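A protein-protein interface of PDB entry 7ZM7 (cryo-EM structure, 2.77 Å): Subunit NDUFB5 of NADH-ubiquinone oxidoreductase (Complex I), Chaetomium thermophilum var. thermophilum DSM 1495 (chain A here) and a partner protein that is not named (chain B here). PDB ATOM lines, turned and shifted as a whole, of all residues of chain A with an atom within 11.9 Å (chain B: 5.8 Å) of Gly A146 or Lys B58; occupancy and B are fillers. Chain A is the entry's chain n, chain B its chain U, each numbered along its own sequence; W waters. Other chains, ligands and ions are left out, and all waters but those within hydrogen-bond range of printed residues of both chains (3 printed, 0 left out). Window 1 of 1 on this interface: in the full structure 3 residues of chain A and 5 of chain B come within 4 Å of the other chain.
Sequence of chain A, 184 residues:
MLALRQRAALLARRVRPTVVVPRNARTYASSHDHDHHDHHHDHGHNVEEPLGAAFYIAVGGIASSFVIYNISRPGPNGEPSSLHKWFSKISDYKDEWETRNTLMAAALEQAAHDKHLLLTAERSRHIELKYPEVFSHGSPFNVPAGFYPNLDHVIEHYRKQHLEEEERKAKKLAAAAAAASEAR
The side-chain amide oxygen (OD1) of Asn B59 lies within hydrogen-bond range of the backbone NH (N) of Gly A146, 2.8 Å away. N of Gly B63 lies within hydrogen-bond range of O of Gly A146, at 3.4 Å.
The side-chain carboxylate (OE2) of Glu B66 is in salt-bridge range of the side-chain amino group (NZ) of Lys B58 (3.5 Å). The backbone NH (N) of Lys B58 sits at hydrogen-bond distance from the side-chain sulfur (SG) of Cys B69, at 3.4 Å. The backbone carbonyl oxygen of Ser A139 sits at hydrogen-bond distance from the side-chain hydroxyl of Tyr A148 (2.8 Å). SG of Cys B57 forms a disulfide with SG of Cys B69, 2.0 Å away.
Met B55 touches Ala A145. CB of Ala A145 touches CB of Lys B58, 3.6 Å away. Ala A145 touches Asn B59 (CA to OD1, 3.3 Å). CA of Gly A146 touches O of Lys B58, 3.3 Å away. Gly A146 touches Pro B62. Tyr A148 touches Pro B62 (O to CB, 3.8 Å).
Pro A144 touches none of the printed residues of chain B. Of the printed residues of chain B, Ala A145 touches Met B55 (3.6 Å), Lys B58 (3.6 Å) and Asn B59 (3.3 Å). Printed residues of chain B within 4 Å of Gly A146: Lys B58, Asn B59, Pro B62 and Gly B63. Of the printed residues of chain B, Tyr A148 touches Pro B62. Asp B53 touches none of the printed residues of chain A. Met B55 touches one residue of chain A. No residue of chain A comes within 4 Å of Cys B57. Of the printed residues of chain A, Lys B58 touches Ala A145 (3.6 Å) and Gly A146 (3.3 Å). Asn B59 touches just these residues of chain A: Ala A145 and Gly A146. No residue of chain A comes within 4 Å of Glu B60. Gly B63 touches one residue of chain A. No residue of chain A comes within 4 Å of Gly B65. Glu B66 touches none of the printed residues of chain A. No residue of chain A comes within 4 Å of Cys B69. The nearest residue of chain A that does not touch Lys B58 is Phe A147 (5.7 Å). The nearest printed residue of chain B that does not touch Ala A145 is Glu B66 (5.3 Å).
Of the 14 printed residues of chain B, 5 touch a printed residue of chain A. Printed residues of chain A that touch a printed residue of chain B: Ala A145, Gly A146 and Tyr A148.
Water W1 lies within hydrogen-bond range of O of Tyr A148 and O of Asn B59. Water W3 bridges the backbone carbonyl oxygen of Gly A146 (2.9 Å) and the backbone NH of Gly B63 (3.0 Å). Water W2 lies within hydrogen-bond range of N of Tyr A148 (3.0 Å) and OD1 of Asn B59 (3.5 Å).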
ATOM      1  N   SER A 139     -14.478 -28.614  17.251  1.00  0.00           N
ATOM      2  CA  SER A 139     -15.271 -29.001  16.056  1.00  0.00           C
ATOM      3  C   SER A 139     -14.820 -28.252  14.802  1.00  0.00           C
ATOM      4  O   SER A 139     -14.637 -27.044  14.870  1.00  0.00           O
ATOM      5  CB  SER A 139     -16.757 -28.849  16.302  1.00  0.00           C
ATOM      6  OG  SER A 139     -17.504 -29.087  15.121  1.00  0.00           O
ATOM      7  N   PHE A 141     -16.784 -27.872  12.197  1.00  0.00           N
ATOM      8  CA  PHE A 141     -18.043 -27.543  11.487  1.00  0.00           C
ATOM      9  C   PHE A 141     -18.809 -26.424  12.170  1.00  0.00           C
ATOM     10  O   PHE A 141     -18.712 -26.332  13.391  1.00  0.00           O
ATOM     11  CB  PHE A 141     -18.980 -28.747  11.530  1.00  0.00           C
ATOM     12  CG  PHE A 141     -18.321 -30.059  11.196  1.00  0.00           C
ATOM     13  CD1 PHE A 141     -17.742 -30.263   9.955  1.00  0.00           C
ATOM     14  CD2 PHE A 141     -18.280 -31.087  12.121  1.00  0.00           C
ATOM     15  CE1 PHE A 141     -17.130 -31.464   9.647  1.00  0.00           C
ATOM     16  CE2 PHE A 141     -17.668 -32.290  11.812  1.00  0.00           C
ATOM     17  CZ  PHE A 141     -17.092 -32.471  10.577  1.00  0.00           C
ATOM     18  N   ASN A 142     -19.501 -25.598  11.388  1.00  0.00           N
ATOM     19  CA  ASN A 142     -20.377 -24.530  11.931  1.00  0.00           C
ATOM     20  C   ASN A 142     -19.539 -23.605  12.784  1.00  0.00           C
ATOM     21  O   ASN A 142     -20.038 -23.139  13.813  1.00  0.00           O
ATOM     22  CB  ASN A 142     -21.622 -25.108  12.605  1.00  0.00           C
ATOM     23  CG  ASN A 142     -22.578 -25.761  11.639  1.00  0.00           C
ATOM     24  OD1 ASN A 142     -22.811 -25.249  10.551  1.00  0.00           O
ATOM     25  ND2 ASN A 142     -23.140 -26.886  12.045  1.00  0.00           N
ATOM     26  N   VAL A 143     -18.314 -23.360  12.345  1.00  0.00           N
ATOM     27  CA  VAL A 143     -17.371 -22.529  13.134  1.00  0.00           C
ATOM     28  C   VAL A 143     -17.666 -21.052  12.864  1.00  0.00           C
ATOM     29  O   VAL A 143     -17.596 -20.667  11.688  1.00  0.00           O
ATOM     30  CB  VAL A 143     -15.919 -22.913  12.815  1.00  0.00           C
ATOM     31  CG1 VAL A 143     -14.931 -22.019  13.542  1.00  0.00           C
ATOM     32  CG2 VAL A 143     -15.649 -24.374  13.119  1.00  0.00           C
ATOM     33  N   PRO A 144     -18.024 -20.202  13.862  1.00  0.00           N
ATOM     34  CA  PRO A 144     -18.182 -18.783  13.572  1.00  0.00           C
ATOM     35  C   PRO A 144     -16.860 -18.015  13.490  1.00  0.00           C
ATOM     36  O   PRO A 144     -15.966 -18.360  14.210  1.00  0.00           O
ATOM     37  CB  PRO A 144     -18.874 -18.278  14.845  1.00  0.00           C
ATOM     38  CG  PRO A 144     -19.279 -19.503  15.638  1.00  0.00           C
ATOM     39  CD  PRO A 144     -18.291 -20.573  15.246  1.00  0.00           C
ATOM     40  N   ALA A 145     -16.744 -17.065  12.571  1.00  0.00           N
ATOM     41  CA  ALA A 145     -15.467 -16.338  12.399  1.00  0.00           C
ATOM     42  C   ALA A 145     -15.039 -15.704  13.726  1.00  0.00           C
ATOM     43  O   ALA A 145     -15.881 -15.060  14.378  1.00  0.00           O
ATOM     44  CB  ALA A 145     -15.568 -15.325  11.295  1.00  0.00           C
ATOM     45  N   GLY A 146     -13.774 -15.864  14.091  1.00  0.00           N
ATOM     46  CA  GLY A 146     -13.258 -15.253  15.322  1.00  0.00           C
ATOM     47  C   GLY A 146     -13.453 -16.133  16.527  1.00  0.00           C
ATOM     48  O   GLY A 146     -13.017 -15.730  17.614  1.00  0.00           O
ATOM     49  N   PHE A 147     -14.103 -17.280  16.372  1.00  0.00           N
ATOM     50  CA  PHE A 147     -14.390 -18.114  17.560  1.00  0.00           C
ATOM     51  C   PHE A 147     -13.091 -18.667  18.123  1.00  0.00           C
ATOM     52  O   PHE A 147     -12.862 -18.524  19.327  1.00  0.00           O
ATOM     53  CB  PHE A 147     -15.350 -19.246  17.191  1.00  0.00           C
ATOM     54  CG  PHE A 147     -15.601 -20.252  18.279  1.00  0.00           C
ATOM     55  CD1 PHE A 147     -14.760 -21.338  18.444  1.00  0.00           C
ATOM     56  CD2 PHE A 147     -16.687 -20.117  19.126  1.00  0.00           C
ATOM     57  CE1 PHE A 147     -14.986 -22.259  19.447  1.00  0.00           C
ATOM     58  CE2 PHE A 147     -16.919 -21.047  20.122  1.00  0.00           C
ATOM     59  CZ  PHE A 147     -16.071 -22.115  20.273  1.00  0.00           C
ATOM     60  N   TYR A 148     -12.250 -19.222  17.259  1.00  0.00           N
ATOM     61  CA  TYR A 148     -11.020 -19.896  17.744  1.00  0.00           C
ATOM     62  C   TYR A 148      -9.917 -18.885  18.009  1.00  0.00           C
ATOM     63  O   TYR A 148      -9.744 -17.954  17.226  1.00  0.00           O
ATOM     64  CB  TYR A 148     -10.587 -21.019  16.806  1.00  0.00           C
ATOM     65  CG  TYR A 148     -11.382 -22.291  16.905  1.00  0.00           C
ATOM     66  CD1 TYR A 148     -11.199 -23.167  17.957  1.00  0.00           C
ATOM     67  CD2 TYR A 148     -12.298 -22.631  15.928  1.00  0.00           C
ATOM     68  CE1 TYR A 148     -11.918 -24.347  18.042  1.00  0.00           C
ATOM     69  CE2 TYR A 148     -13.024 -23.806  15.996  1.00  0.00           C
ATOM     70  CZ  TYR A 148     -12.833 -24.665  17.058  1.00  0.00           C
ATOM     71  OH  TYR A 148     -13.559 -25.810  17.132  1.00  0.00           O
ATOM     72  N   PRO A 149      -9.164 -19.052  19.110  1.00  0.00           N
ATOM     73  CA  PRO A 149      -8.101 -18.129  19.461  1.00  0.00           C
ATOM     74  C   PRO A 149      -6.804 -18.268  18.665  1.00  0.00           C
ATOM     75  O   PRO A 149      -6.566 -19.302  18.099  1.00  0.00           O
ATOM     76  CB  PRO A 149      -7.887 -18.419  20.949  1.00  0.00           C
ATOM     77  CG  PRO A 149      -8.268 -19.865  21.121  1.00  0.00           C
ATOM     78  CD  PRO A 149      -9.367 -20.103  20.110  1.00  0.00           C
ATOM     79  N   ASN A 150      -6.048 -17.184  18.577  1.00  0.00           N
ATOM     80  CA  ASN A 150      -4.738 -17.217  17.888  1.00  0.00           C
ATOM     81  C   ASN A 150      -3.731 -17.887  18.816  1.00  0.00           C
ATOM     82  O   ASN A 150      -3.282 -17.233  19.766  1.00  0.00           O
ATOM     83  CB  ASN A 150      -4.246 -15.819  17.526  1.00  0.00           C
ATOM     84  CG  ASN A 150      -2.982 -15.851  16.697  1.00  0.00           C
ATOM     85  OD1 ASN A 150      -1.956 -15.309  17.098  1.00  0.00           O
ATOM     86  ND2 ASN A 150      -3.046 -16.494  15.544  1.00  0.00           N
ATOM     87  N   LEU A 151      -3.409 -19.144  18.549  1.00  0.00           N
ATOM     88  CA  LEU A 151      -2.456 -19.891  19.371  1.00  0.00           C
ATOM     89  C   LEU A 151      -1.173 -20.239  18.616  1.00  0.00           C
ATOM     90  O   LEU A 151      -0.727 -21.375  18.605  1.00  0.00           O
ATOM     91  CB  LEU A 151      -3.116 -21.145  19.940  1.00  0.00           C
ATOM     92  CG  LEU A 151      -4.523 -20.900  20.477  1.00  0.00           C
ATOM     93  CD1 LEU A 151      -5.233 -22.200  20.762  1.00  0.00           C
ATOM     94  CD2 LEU A 151      -4.481 -20.003  21.708  1.00  0.00           C
ATOM     95  N   ASP B  53     -13.263 -10.959   2.907  1.00  0.00           N
ATOM     96  CA  ASP B  53     -12.484  -9.991   3.714  1.00  0.00           C
ATOM     97  C   ASP B  53     -13.171  -9.814   5.064  1.00  0.00           C
ATOM     98  O   ASP B  53     -12.468  -9.769   6.082  1.00  0.00           O
ATOM     99  CB  ASP B  53     -12.375  -8.651   2.997  1.00  0.00           C
ATOM    100  CG  ASP B  53     -11.407  -7.683   3.643  1.00  0.00           C
ATOM    101  OD1 ASP B  53     -10.293  -8.113   3.975  1.00  0.00           O
ATOM    102  OD2 ASP B  53     -11.783  -6.510   3.803  1.00  0.00           O
ATOM    103  N   TYR B  54     -14.497  -9.714   5.064  1.00  0.00           N
ATOM    104  CA  TYR B  54     -15.255  -9.495   6.320  1.00  0.00           C
ATOM    105  C   TYR B  54     -15.054 -10.681   7.246  1.00  0.00           C
ATOM    106  O   TYR B  54     -14.936 -10.484   8.456  1.00  0.00           O
ATOM    107  CB  TYR B  54     -16.739  -9.288   6.038  1.00  0.00           C
ATOM    108  CG  TYR B  54     -17.625  -9.282   7.256  1.00  0.00           C
ATOM    109  CD1 TYR B  54     -17.572  -8.244   8.170  1.00  0.00           C
ATOM    110  CD2 TYR B  54     -18.510 -10.316   7.496  1.00  0.00           C
ATOM    111  CE1 TYR B  54     -18.379  -8.233   9.292  1.00  0.00           C
ATOM    112  CE2 TYR B  54     -19.327 -10.320   8.612  1.00  0.00           C
ATOM    113  CZ  TYR B  54     -19.258  -9.276   9.512  1.00  0.00           C
ATOM    114  OH  TYR B  54     -20.061  -9.274  10.611  1.00  0.00           O
ATOM    115  N   MET B  55     -14.968 -11.870   6.678  1.00  0.00           N
ATOM    116  CA  MET B  55     -14.895 -13.090   7.511  1.00  0.00           C
ATOM    117  C   MET B  55     -13.456 -13.244   7.951  1.00  0.00           C
ATOM    118  O   MET B  55     -13.228 -13.784   9.029  1.00  0.00           O
ATOM    119  CB  MET B  55     -15.342 -14.304   6.691  1.00  0.00           C
ATOM    120  CG  MET B  55     -16.810 -14.262   6.343  1.00  0.00           C
ATOM    121  SD  MET B  55     -17.863 -14.288   7.804  1.00  0.00           S
ATOM    122  CE  MET B  55     -17.647 -15.987   8.326  1.00  0.00           C
ATOM    123  N   GLN B  56     -12.535 -12.689   7.171  1.00  0.00           N
ATOM    124  CA  GLN B  56     -11.131 -12.731   7.562  1.00  0.00           C
ATOM    125  C   GLN B  56     -10.813 -11.737   8.672  1.00  0.00           C
ATOM    126  O   GLN B  56     -10.076 -12.060   9.604  1.00  0.00           O
ATOM    127  CB  GLN B  56     -10.272 -12.460   6.342  1.00  0.00           C
ATOM    128  CG  GLN B  56      -9.778 -13.683   5.665  1.00  0.00           C
ATOM    129  CD  GLN B  56      -8.779 -13.352   4.606  1.00  0.00           C
ATOM    130  OE1 GLN B  56      -8.985 -12.439   3.822  1.00  0.00           O
ATOM    131  NE2 GLN B  56      -7.685 -14.091   4.572  1.00  0.00           N
ATOM    132  N   CYS B  57     -11.299 -10.503   8.547  1.00  0.00           N
ATOM    133  CA  CYS B  57     -11.124  -9.488   9.624  1.00  0.00           C
ATOM    134  C   CYS B  57     -11.602 -10.085  10.942  1.00  0.00           C
ATOM    135  O   CYS B  57     -10.926  -9.878  11.952  1.00  0.00           O
ATOM    136  CB  CYS B  57     -11.962  -8.242   9.348  1.00  0.00           C
ATOM    137  SG  CYS B  57     -11.962  -6.989  10.661  1.00  0.00           S
ATOM    138  N   LYS B  58     -12.756 -10.747  10.945  1.00  0.00           N
ATOM    139  CA  LYS B  58     -13.322 -11.294  12.205  1.00  0.00           C
ATOM    140  C   LYS B  58     -12.413 -12.400  12.734  1.00  0.00           C
ATOM    141  O   LYS B  58     -12.196 -12.442  13.946  1.00  0.00           O
ATOM    142  CB  LYS B  58     -14.721 -11.849  11.942  1.00  0.00           C
ATOM    143  CG  LYS B  58     -15.798 -10.825  11.626  1.00  0.00           C
ATOM    144  CD  LYS B  58     -17.144 -11.465  11.406  1.00  0.00           C
ATOM    145  CE  LYS B  58     -17.674 -12.175  12.632  1.00  0.00           C
ATOM    146  NZ  LYS B  58     -17.850 -11.246  13.771  1.00  0.00           N
ATOM    147  N   ASN B  59     -11.929 -13.264  11.849  1.00  0.00           N
ATOM    148  CA  ASN B  59     -11.003 -14.352  12.233  1.00  0.00           C
ATOM    149  C   ASN B  59      -9.710 -13.734  12.752  1.00  0.00           C
ATOM    150  O   ASN B  59      -9.133 -14.296  13.692  1.00  0.00           O
ATOM    151  CB  ASN B  59     -10.698 -15.264  11.048  1.00  0.00           C
ATOM    152  CG  ASN B  59     -11.300 -16.643  11.181  1.00  0.00           C
ATOM    153  OD1 ASN B  59     -12.258 -16.838  11.919  1.00  0.00           O
ATOM    154  ND2 ASN B  59     -10.741 -17.606  10.470  1.00  0.00           N
ATOM    155  N   GLU B  60      -9.254 -12.645  12.138  1.00  0.00           N
ATOM    156  CA  GLU B  60      -7.983 -11.991  12.553  1.00  0.00           C
ATOM    157  C   GLU B  60      -8.100 -11.482  13.990  1.00  0.00           C
ATOM    158  O   GLU B  60      -7.082 -11.516  14.700  1.00  0.00           O
ATOM    159  CB  GLU B  60      -7.562 -10.882  11.593  1.00  0.00           C
ATOM    160  CG  GLU B  60      -6.786 -11.388  10.393  1.00  0.00           C
ATOM    161  CD  GLU B  60      -6.145 -10.288   9.566  1.00  0.00           C
ATOM    162  OE1 GLU B  60      -6.489  -9.110   9.784  1.00  0.00           O
ATOM    163  OE2 GLU B  60      -5.298 -10.612   8.709  1.00  0.00           O
ATOM    164  N   ASN B  61      -9.273 -10.994  14.394  1.00  0.00           N
ATOM    165  CA  ASN B  61      -9.413 -10.396  15.738  1.00  0.00           C
ATOM    166  C   ASN B  61     -10.380 -11.243  16.555  1.00  0.00           C
ATOM    167  O   ASN B  61     -11.565 -10.882  16.635  1.00  0.00           O
ATOM    168  CB  ASN B  61      -9.957  -8.970  15.655  1.00  0.00           C
ATOM    169  CG  ASN B  61      -9.170  -8.075  14.725  1.00  0.00           C
ATOM    170  OD1 ASN B  61      -9.469  -7.986  13.538  1.00  0.00           O
ATOM    171  ND2 ASN B  61      -8.165  -7.399  15.259  1.00  0.00           N
ATOM    172  N   PRO B  62      -9.911 -12.301  17.241  1.00  0.00           N
ATOM    173  CA  PRO B  62     -10.802 -13.187  17.979  1.00  0.00           C
ATOM    174  C   PRO B  62     -11.503 -12.507  19.168  1.00  0.00           C
ATOM    175  O   PRO B  62     -10.937 -11.584  19.706  1.00  0.00           O
ATOM    176  CB  PRO B  62      -9.864 -14.339  18.380  1.00  0.00           C
ATOM    177  CG  PRO B  62      -8.694 -14.224  17.442  1.00  0.00           C
ATOM    178  CD  PRO B  62      -8.519 -12.731  17.300  1.00  0.00           C
ATOM    179  N   GLY B  63     -12.694 -12.976  19.544  1.00  0.00           N
ATOM    180  CA  GLY B  63     -13.464 -12.422  20.675  1.00  0.00           C
ATOM    181  C   GLY B  63     -13.777 -10.942  20.589  1.00  0.00           C
ATOM    182  O   GLY B  63     -14.480 -10.464  21.476  1.00  0.00           O
ATOM    183  N   GLY B  65     -14.490  -9.332  17.355  1.00  0.00           N
ATOM    184  CA  GLY B  65     -14.770  -9.087  15.931  1.00  0.00           C
ATOM    185  C   GLY B  65     -16.115  -8.507  15.600  1.00  0.00           C
ATOM    186  O   GLY B  65     -16.272  -8.124  14.440  1.00  0.00           O
ATOM    187  N   GLU B  66     -17.071  -8.468  16.528  1.00  0.00           N
ATOM    188  CA  GLU B  66     -18.330  -7.773  16.178  1.00  0.00           C
ATOM    189  C   GLU B  66     -17.931  -6.301  16.108  1.00  0.00           C
ATOM    190  O   GLU B  66     -18.279  -5.649  15.129  1.00  0.00           O
ATOM    191  CB  GLU B  66     -19.381  -8.113  17.239  1.00  0.00           C
ATOM    192  CG  GLU B  66     -19.870  -9.548  17.185  1.00  0.00           C
ATOM    193  CD  GLU B  66     -18.875 -10.632  17.568  1.00  0.00           C
ATOM    194  OE1 GLU B  66     -17.949 -10.344  18.358  1.00  0.00           O
ATOM    195  OE2 GLU B  66     -19.022 -11.764  17.063  1.00  0.00           O
ATOM    196  N   CYS B  69     -14.604  -4.828  13.281  1.00  0.00           N
ATOM    197  CA  CYS B  69     -14.815  -5.294  11.884  1.00  0.00           C
ATOM    198  C   CYS B  69     -16.069  -4.609  11.339  1.00  0.00           C
ATOM    199  O   CYS B  69     -16.627  -5.124  10.384  1.00  0.00           O
ATOM    200  CB  CYS B  69     -14.850  -6.815  11.773  1.00  0.00           C
ATOM    201  SG  CYS B  69     -13.256  -7.595  12.130  1.00  0.00           S
HETATM  202  O   HOH W   1     -10.164 -16.499  15.022  1.00  0.00           O
HETATM  203  O   HOH W   2     -12.243 -19.433  14.244  1.00  0.00           O
HETATM  204  O   HOH W   3     -15.124 -13.869  18.128  1.00  0.00           O
